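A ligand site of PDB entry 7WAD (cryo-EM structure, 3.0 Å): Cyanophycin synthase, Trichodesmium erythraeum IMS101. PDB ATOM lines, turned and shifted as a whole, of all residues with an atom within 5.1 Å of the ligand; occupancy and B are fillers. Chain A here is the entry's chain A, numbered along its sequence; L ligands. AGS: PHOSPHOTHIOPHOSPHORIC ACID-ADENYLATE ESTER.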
ATOM      1  N   LYS A 220      -3.413 -21.267 -11.094  1.00  0.00           N
ATOM      2  CA  LYS A 220      -4.388 -20.211 -11.338  1.00  0.00           C
ATOM      3  C   LYS A 220      -5.217 -20.493 -12.575  1.00  0.00           C
ATOM      4  O   LYS A 220      -6.460 -20.381 -12.549  1.00  0.00           O
ATOM      5  CB  LYS A 220      -3.664 -18.871 -11.473  1.00  0.00           C
ATOM      6  CG  LYS A 220      -2.857 -18.471 -10.254  1.00  0.00           C
ATOM      7  CD  LYS A 220      -3.681 -18.583  -8.980  1.00  0.00           C
ATOM      8  CE  LYS A 220      -2.803 -18.442  -7.744  1.00  0.00           C
ATOM      9  NZ  LYS A 220      -3.499 -18.906  -6.513  1.00  0.00           N
ATOM     10  N   PRO A 235     -13.203 -13.495 -13.823  1.00  0.00           N
ATOM     11  CA  PRO A 235     -12.808 -12.469 -14.795  1.00  0.00           C
ATOM     12  C   PRO A 235     -12.564 -13.055 -16.172  1.00  0.00           C
ATOM     13  O   PRO A 235     -12.034 -14.156 -16.328  1.00  0.00           O
ATOM     14  CB  PRO A 235     -11.508 -11.896 -14.200  1.00  0.00           C
ATOM     15  CG  PRO A 235     -11.026 -12.941 -13.263  1.00  0.00           C
ATOM     16  CD  PRO A 235     -12.255 -13.566 -12.695  1.00  0.00           C
ATOM     17  N   VAL A 259      -5.750  -5.664 -17.386  1.00  0.00           N
ATOM     18  CA  VAL A 259      -4.723  -6.045 -16.423  1.00  0.00           C
ATOM     19  C   VAL A 259      -3.769  -7.003 -17.103  1.00  0.00           C
ATOM     20  O   VAL A 259      -4.183  -7.949 -17.766  1.00  0.00           O
ATOM     21  CB  VAL A 259      -5.342  -6.698 -15.165  1.00  0.00           C
ATOM     22  CG1 VAL A 259      -4.257  -7.069 -14.177  1.00  0.00           C
ATOM     23  CG2 VAL A 259      -6.368  -5.769 -14.533  1.00  0.00           C
ATOM     24  N   LYS A 261      -0.632  -9.619 -16.479  1.00  0.00           N
ATOM     25  CA  LYS A 261       0.010 -10.396 -15.440  1.00  0.00           C
ATOM     26  C   LYS A 261       0.775 -11.562 -16.048  1.00  0.00           C
ATOM     27  O   LYS A 261       0.493 -11.973 -17.180  1.00  0.00           O
ATOM     28  CB  LYS A 261      -1.007 -10.934 -14.421  1.00  0.00           C
ATOM     29  CG  LYS A 261      -2.083 -11.827 -15.009  1.00  0.00           C
ATOM     30  CD  LYS A 261      -2.828 -12.568 -13.915  1.00  0.00           C
ATOM     31  CE  LYS A 261      -3.692 -11.618 -13.095  1.00  0.00           C
ATOM     32  NZ  LYS A 261      -4.565 -12.337 -12.128  1.00  0.00           N
ATOM     33  N   GLY A 265       4.391 -16.317 -11.056  1.00  0.00           N
ATOM     34  CA  GLY A 265       5.141 -15.282 -10.374  1.00  0.00           C
ATOM     35  C   GLY A 265       4.883 -15.336  -8.886  1.00  0.00           C
ATOM     36  O   GLY A 265       3.857 -15.843  -8.430  1.00  0.00           O
ATOM     37  N   ASN A 266       5.834 -14.792  -8.129  1.00  0.00           N
ATOM     38  CA  ASN A 266       5.753 -14.722  -6.679  1.00  0.00           C
ATOM     39  C   ASN A 266       5.950 -13.279  -6.237  1.00  0.00           C
ATOM     40  O   ASN A 266       6.717 -12.538  -6.857  1.00  0.00           O
ATOM     41  CB  ASN A 266       6.778 -15.652  -6.018  1.00  0.00           C
ATOM     42  CG  ASN A 266       8.162 -15.541  -6.647  1.00  0.00           C
ATOM     43  OD1 ASN A 266       8.616 -14.462  -7.019  1.00  0.00           O
ATOM     44  ND2 ASN A 266       8.849 -16.681  -6.756  1.00  0.00           N
ATOM     45  N   HIS A 267       5.222 -12.881  -5.193  1.00  0.00           N
ATOM     46  CA  HIS A 267       5.273 -11.531  -4.646  1.00  0.00           C
ATOM     47  C   HIS A 267       4.893 -10.473  -5.685  1.00  0.00           C
ATOM     48  O   HIS A 267       5.380  -9.337  -5.624  1.00  0.00           O
ATOM     49  CB  HIS A 267       6.657 -11.225  -4.044  1.00  0.00           C
ATOM     50  CG  HIS A 267       6.689 -10.013  -3.172  1.00  0.00           C
ATOM     51  ND1 HIS A 267       5.897  -9.885  -2.047  1.00  0.00           N
ATOM     52  CD2 HIS A 267       7.426  -8.872  -3.248  1.00  0.00           C
ATOM     53  CE1 HIS A 267       6.147  -8.716  -1.473  1.00  0.00           C
ATOM     54  NE2 HIS A 267       7.062  -8.091  -2.188  1.00  0.00           N
ATOM     55  N   GLY A 268       4.034 -10.837  -6.633  1.00  0.00           N
ATOM     56  CA  GLY A 268       3.554  -9.896  -7.624  1.00  0.00           C
ATOM     57  C   GLY A 268       4.621  -9.346  -8.558  1.00  0.00           C
ATOM     58  O   GLY A 268       4.676  -8.139  -8.799  1.00  0.00           O
ATOM     59  N   ILE A 271       3.482  -7.452 -12.601  1.00  0.00           N
ATOM     60  CA  ILE A 271       2.038  -7.398 -12.759  1.00  0.00           C
ATOM     61  C   ILE A 271       1.588  -5.951 -12.598  1.00  0.00           C
ATOM     62  O   ILE A 271       1.920  -5.296 -11.599  1.00  0.00           O
ATOM     63  CB  ILE A 271       1.310  -8.324 -11.773  1.00  0.00           C
ATOM     64  CG1 ILE A 271      -0.211  -8.144 -11.880  1.00  0.00           C
ATOM     65  CG2 ILE A 271       1.803  -8.090 -10.345  1.00  0.00           C
ATOM     66  CD1 ILE A 271      -1.000  -9.187 -11.130  1.00  0.00           C
ATOM     67  N   ILE A 273      -1.741  -3.137 -12.526  1.00  0.00           N
ATOM     68  CA  ILE A 273      -3.079  -3.109 -11.954  1.00  0.00           C
ATOM     69  C   ILE A 273      -4.081  -2.452 -12.898  1.00  0.00           C
ATOM     70  O   ILE A 273      -5.125  -3.033 -13.201  1.00  0.00           O
ATOM     71  CB  ILE A 273      -3.068  -2.396 -10.580  1.00  0.00           C
ATOM     72  CG1 ILE A 273      -2.086  -3.094  -9.644  1.00  0.00           C
ATOM     73  CG2 ILE A 273      -4.458  -2.381  -9.977  1.00  0.00           C
ATOM     74  CD1 ILE A 273      -2.427  -4.534  -9.353  1.00  0.00           C
ATOM     75  N   GLU A 300      -6.302  -9.780 -18.516  1.00  0.00           N
ATOM     76  CA  GLU A 300      -7.677  -9.860 -18.053  1.00  0.00           C
ATOM     77  C   GLU A 300      -8.358  -8.508 -18.244  1.00  0.00           C
ATOM     78  O   GLU A 300      -7.705  -7.486 -18.434  1.00  0.00           O
ATOM     79  CB  GLU A 300      -7.803 -10.241 -16.575  1.00  0.00           C
ATOM     80  CG  GLU A 300      -7.369 -11.643 -16.193  1.00  0.00           C
ATOM     81  CD  GLU A 300      -5.874 -11.748 -15.990  1.00  0.00           C
ATOM     82  OE1 GLU A 300      -5.171 -10.723 -16.080  1.00  0.00           O
ATOM     83  OE2 GLU A 300      -5.416 -12.865 -15.675  1.00  0.00           O
ATOM     84  N   ARG A 301      -9.686  -8.532 -18.186  1.00  0.00           N
ATOM     85  CA  ARG A 301     -10.433  -7.302 -17.980  1.00  0.00           C
ATOM     86  C   ARG A 301     -10.243  -6.824 -16.548  1.00  0.00           C
ATOM     87  O   ARG A 301     -10.145  -7.624 -15.621  1.00  0.00           O
ATOM     88  CB  ARG A 301     -11.920  -7.533 -18.272  1.00  0.00           C
ATOM     89  CG  ARG A 301     -12.799  -6.335 -17.993  1.00  0.00           C
ATOM     90  CD  ARG A 301     -14.208  -6.753 -17.607  1.00  0.00           C
ATOM     91  NE  ARG A 301     -15.186  -5.713 -17.899  1.00  0.00           N
ATOM     92  CZ  ARG A 301     -15.309  -4.587 -17.197  1.00  0.00           C
ATOM     93  NH1 ARG A 301     -14.535  -4.330 -16.162  1.00  0.00           N
ATOM     94  NH2 ARG A 301     -16.243  -3.711 -17.546  1.00  0.00           N
ATOM     95  N   TYR A 302     -10.188  -5.513 -16.372  1.00  0.00           N
ATOM     96  CA  TYR A 302     -10.025  -4.923 -15.045  1.00  0.00           C
ATOM     97  C   TYR A 302     -11.382  -4.722 -14.405  1.00  0.00           C
ATOM     98  O   TYR A 302     -12.290  -4.147 -15.013  1.00  0.00           O
ATOM     99  CB  TYR A 302      -9.275  -3.598 -15.123  1.00  0.00           C
ATOM    100  CG  TYR A 302      -9.148  -2.902 -13.782  1.00  0.00           C
ATOM    101  CD1 TYR A 302      -8.244  -3.349 -12.836  1.00  0.00           C
ATOM    102  CD2 TYR A 302      -9.931  -1.803 -13.468  1.00  0.00           C
ATOM    103  CE1 TYR A 302      -8.127  -2.722 -11.607  1.00  0.00           C
ATOM    104  CE2 TYR A 302      -9.814  -1.167 -12.255  1.00  0.00           C
ATOM    105  CZ  TYR A 302      -8.909  -1.630 -11.324  1.00  0.00           C
ATOM    106  OH  TYR A 302      -8.800  -0.999 -10.107  1.00  0.00           O
ATOM    107  N   TYR A 303     -11.529  -5.206 -13.169  1.00  0.00           N
ATOM    108  CA  TYR A 303     -12.764  -5.097 -12.411  1.00  0.00           C
ATOM    109  C   TYR A 303     -12.558  -4.141 -11.253  1.00  0.00           C
ATOM    110  O   TYR A 303     -11.621  -4.312 -10.462  1.00  0.00           O
ATOM    111  CB  TYR A 303     -13.221  -6.464 -11.908  1.00  0.00           C
ATOM    112  CG  TYR A 303     -13.841  -7.330 -12.981  1.00  0.00           C
ATOM    113  CD1 TYR A 303     -15.193  -7.262 -13.260  1.00  0.00           C
ATOM    114  CD2 TYR A 303     -13.054  -8.195 -13.720  1.00  0.00           C
ATOM    115  CE1 TYR A 303     -15.757  -8.047 -14.239  1.00  0.00           C
ATOM    116  CE2 TYR A 303     -13.615  -8.992 -14.705  1.00  0.00           C
ATOM    117  CZ  TYR A 303     -14.960  -8.911 -14.957  1.00  0.00           C
ATOM    118  OH  TYR A 303     -15.524  -9.696 -15.936  1.00  0.00           O
ATOM    119  N   ASP A 307     -11.540  -5.209  -2.517  1.00  0.00           N
ATOM    120  CA  ASP A 307     -11.048  -6.564  -2.357  1.00  0.00           C
ATOM    121  C   ASP A 307     -11.523  -7.150  -1.043  1.00  0.00           C
ATOM    122  O   ASP A 307     -11.352  -6.548   0.024  1.00  0.00           O
ATOM    123  CB  ASP A 307      -9.523  -6.570  -2.427  1.00  0.00           C
ATOM    124  CG  ASP A 307      -8.946  -7.967  -2.508  1.00  0.00           C
ATOM    125  OD1 ASP A 307      -9.004  -8.574  -3.601  1.00  0.00           O
ATOM    126  OD2 ASP A 307      -8.436  -8.462  -1.481  1.00  0.00           O
ATOM    127  N   ARG A 323     -10.234  -5.649   2.713  1.00  0.00           N
ATOM    128  CA  ARG A 323      -8.926  -5.034   2.863  1.00  0.00           C
ATOM    129  C   ARG A 323      -8.961  -3.610   2.310  1.00  0.00           C
ATOM    130  O   ARG A 323      -9.119  -3.418   1.101  1.00  0.00           O
ATOM    131  CB  ARG A 323      -7.857  -5.849   2.141  1.00  0.00           C
ATOM    132  CG  ARG A 323      -7.365  -7.051   2.913  1.00  0.00           C
ATOM    133  CD  ARG A 323      -8.122  -8.306   2.547  1.00  0.00           C
ATOM    134  NE  ARG A 323      -7.780  -8.774   1.213  1.00  0.00           N
ATOM    135  CZ  ARG A 323      -6.762  -9.572   0.942  1.00  0.00           C
ATOM    136  NH1 ARG A 323      -5.951 -10.010   1.885  1.00  0.00           N
ATOM    137  NH2 ARG A 323      -6.538  -9.936  -0.321  1.00  0.00           N
ATOM    138  N   THR A 392      -2.538  -1.819  -3.785  1.00  0.00           N
ATOM    139  CA  THR A 392      -2.574  -3.278  -3.790  1.00  0.00           C
ATOM    140  C   THR A 392      -3.547  -3.848  -2.768  1.00  0.00           C
ATOM    141  O   THR A 392      -3.939  -5.014  -2.894  1.00  0.00           O
ATOM    142  CB  THR A 392      -1.176  -3.839  -3.544  1.00  0.00           C
ATOM    143  OG1 THR A 392      -1.129  -5.217  -3.955  1.00  0.00           O
ATOM    144  CG2 THR A 392      -0.798  -3.747  -2.075  1.00  0.00           C
ATOM    145  N   ASP A 431     -10.567 -14.915  -2.645  1.00  0.00           N
ATOM    146  CA  ASP A 431     -10.456 -13.490  -2.916  1.00  0.00           C
ATOM    147  C   ASP A 431     -11.587 -13.071  -3.848  1.00  0.00           C
ATOM    148  O   ASP A 431     -11.775 -13.681  -4.906  1.00  0.00           O
ATOM    149  CB  ASP A 431      -9.099 -13.155  -3.534  1.00  0.00           C
ATOM    150  CG  ASP A 431      -7.979 -13.219  -2.523  1.00  0.00           C
ATOM    151  OD1 ASP A 431      -8.220 -13.674  -1.391  1.00  0.00           O
ATOM    152  OD2 ASP A 431      -6.849 -12.817  -2.863  1.00  0.00           O
ATOM    153  N   VAL A 433     -13.672  -9.648  -5.722  1.00  0.00           N
ATOM    154  CA  VAL A 433     -13.640  -8.248  -6.098  1.00  0.00           C
ATOM    155  C   VAL A 433     -15.064  -7.857  -6.471  1.00  0.00           C
ATOM    156  O   VAL A 433     -15.581  -8.278  -7.515  1.00  0.00           O
ATOM    157  CB  VAL A 433     -12.662  -7.978  -7.249  1.00  0.00           C
ATOM    158  CG1 VAL A 433     -12.822  -6.557  -7.734  1.00  0.00           C
ATOM    159  CG2 VAL A 433     -11.248  -8.225  -6.795  1.00  0.00           C
ATOM    160  N   VAL A 449     -11.370 -14.020  -7.738  1.00  0.00           N
ATOM    161  CA  VAL A 449     -10.031 -13.802  -8.248  1.00  0.00           C
ATOM    162  C   VAL A 449      -9.130 -15.009  -8.036  1.00  0.00           C
ATOM    163  O   VAL A 449      -8.519 -15.499  -8.994  1.00  0.00           O
ATOM    164  CB  VAL A 449      -9.421 -12.535  -7.598  1.00  0.00           C
ATOM    165  CG1 VAL A 449      -7.916 -12.568  -7.708  1.00  0.00           C
ATOM    166  CG2 VAL A 449      -9.966 -11.301  -8.269  1.00  0.00           C
ATOM    167  N   GLU A 450      -9.030 -15.525  -6.814  1.00  0.00           N
ATOM    168  CA  GLU A 450      -8.157 -16.662  -6.561  1.00  0.00           C
ATOM    169  C   GLU A 450      -8.600 -17.379  -5.294  1.00  0.00           C
ATOM    170  O   GLU A 450      -9.381 -16.868  -4.497  1.00  0.00           O
ATOM    171  CB  GLU A 450      -6.689 -16.227  -6.456  1.00  0.00           C
ATOM    172  CG  GLU A 450      -6.361 -15.457  -5.203  1.00  0.00           C
ATOM    173  CD  GLU A 450      -4.875 -15.451  -4.904  1.00  0.00           C
ATOM    174  OE1 GLU A 450      -4.222 -16.492  -5.144  1.00  0.00           O
ATOM    175  OE2 GLU A 450      -4.358 -14.419  -4.435  1.00  0.00           O
ATOM    176  N   ASN A 452      -6.903 -19.779  -2.061  1.00  0.00           N
ATOM    177  CA  ASN A 452      -5.699 -20.163  -1.337  1.00  0.00           C
ATOM    178  C   ASN A 452      -6.004 -21.347  -0.425  1.00  0.00           C
ATOM    179  O   ASN A 452      -7.019 -21.355   0.276  1.00  0.00           O
ATOM    180  CB  ASN A 452      -5.158 -18.989  -0.509  1.00  0.00           C
ATOM    181  CG  ASN A 452      -4.960 -17.742  -1.344  1.00  0.00           C
ATOM    182  OD1 ASN A 452      -5.791 -16.845  -1.330  1.00  0.00           O
ATOM    183  ND2 ASN A 452      -3.842 -17.678  -2.053  1.00  0.00           N
HETATM  184  PG  AGS L   1       0.798 -13.841  -4.471  1.00  0.00           P
HETATM  185  S1G AGS L   1       0.607 -12.675  -2.925  1.00  0.00           S
HETATM  186  O2G AGS L   1      -0.378 -14.875  -4.484  1.00  0.00           O
HETATM  187  O3G AGS L   1       2.150 -14.611  -4.385  1.00  0.00           O
HETATM  188  PB  AGS L   1       0.088 -13.602  -7.081  1.00  0.00           P
HETATM  189  O1B AGS L   1       0.834 -13.186  -8.290  1.00  0.00           O
HETATM  190  O2B AGS L   1       0.088 -15.127  -6.893  1.00  0.00           O
HETATM  191  O3B AGS L   1       0.755 -12.997  -5.778  1.00  0.00           O
HETATM  192  PA  AGS L   1      -2.009 -12.113  -6.139  1.00  0.00           P
HETATM  193  O1A AGS L   1      -1.133 -10.928  -6.021  1.00  0.00           O
HETATM  194  O2A AGS L   1      -2.255 -12.856  -4.830  1.00  0.00           O
HETATM  195  O3A AGS L   1      -1.429 -13.165  -7.179  1.00  0.00           O
HETATM  196  O5' AGS L   1      -3.360 -11.622  -6.798  1.00  0.00           O
HETATM  197  C5' AGS L   1      -3.387 -10.481  -7.671  1.00  0.00           C
HETATM  198  C4' AGS L   1      -4.163  -9.380  -7.005  1.00  0.00           C
HETATM  199  O4' AGS L   1      -4.451  -8.346  -7.965  1.00  0.00           O
HETATM  200  C3' AGS L   1      -5.513  -9.801  -6.439  1.00  0.00           C
HETATM  201  O3' AGS L   1      -5.386 -10.221  -5.087  1.00  0.00           O
HETATM  202  C2' AGS L   1      -6.345  -8.517  -6.557  1.00  0.00           C
HETATM  203  O2' AGS L   1      -6.109  -7.635  -5.462  1.00  0.00           O
HETATM  204  C1' AGS L   1      -5.790  -7.920  -7.851  1.00  0.00           C
HETATM  205  N9  AGS L   1      -6.511  -8.341  -9.047  1.00  0.00           N
HETATM  206  C8  AGS L   1      -6.189  -9.374  -9.893  1.00  0.00           C
HETATM  207  N7  AGS L   1      -7.011  -9.518 -10.902  1.00  0.00           N
HETATM  208  C5  AGS L   1      -7.945  -8.511 -10.710  1.00  0.00           C
HETATM  209  C6  AGS L   1      -9.082  -8.121 -11.443  1.00  0.00           C
HETATM  210  N6  AGS L   1      -9.497  -8.731 -12.557  1.00  0.00           N
HETATM  211  N1  AGS L   1      -9.793  -7.065 -10.988  1.00  0.00           N
HETATM  212  C2  AGS L   1      -9.383  -6.447  -9.877  1.00  0.00           C
HETATM  213  N3  AGS L   1      -8.327  -6.716  -9.102  1.00  0.00           N
HETATM  214  C4  AGS L   1      -7.641  -7.773  -9.584  1.00  0.00           C
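O2A of the ligand lies close to OE2 of Glu 450, at 2.6 Å.
N of Tyr 303 sits at hydrogen-bond distance from N1 of the ligand, at 3.4 Å.
N6 of the ligand sits at hydrogen-bond distance from O of Arg 301 (3.3 Å).
The side-chain carboxylate of Asp 431 lies within salt-bridge range of the guanidinium group of Arg 323, 3.9 Å away.
The backbone NH (N) of Val 449 lies within hydrogen-bond range of the backbone carbonyl oxygen (O) of Asp 431.
O of Glu 450 sits at hydrogen-bond distance from N of Asp 431, 2.9 Å away.
The side-chain carboxylate (OE1) of Glu 450 lies within hydrogen-bond range of the side-chain amide nitrogen (ND2) of Asn 452.
The side-chain amino group (NZ) of Lys 261 is in salt-bridge range of the side-chain carboxylate (OE2) of Glu 300 (3.7 Å).
OE1 of Glu 450 is in salt-bridge range of NZ of Lys 220.
The guanidinium group of Arg 323 is in salt-bridge range of the side-chain carboxylate of Asp 307 (2.7 Å).
Merely in contact with the ligand: Lys 261 (3.9 Å), His 267 (3.6 Å), Asp 307 (3.6 Å), Asp 431 (3.7 Å) and Val 449 (3.9 Å).
Hydrophobic or aromatic side chains that line the ligand: Tyr 303 and Val 449.
Of the 22 residues printed, 8 come within 4 Å of the ligand.
The nearest printed residue that does not touch the ligand is Val 433 (4.02 Å).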
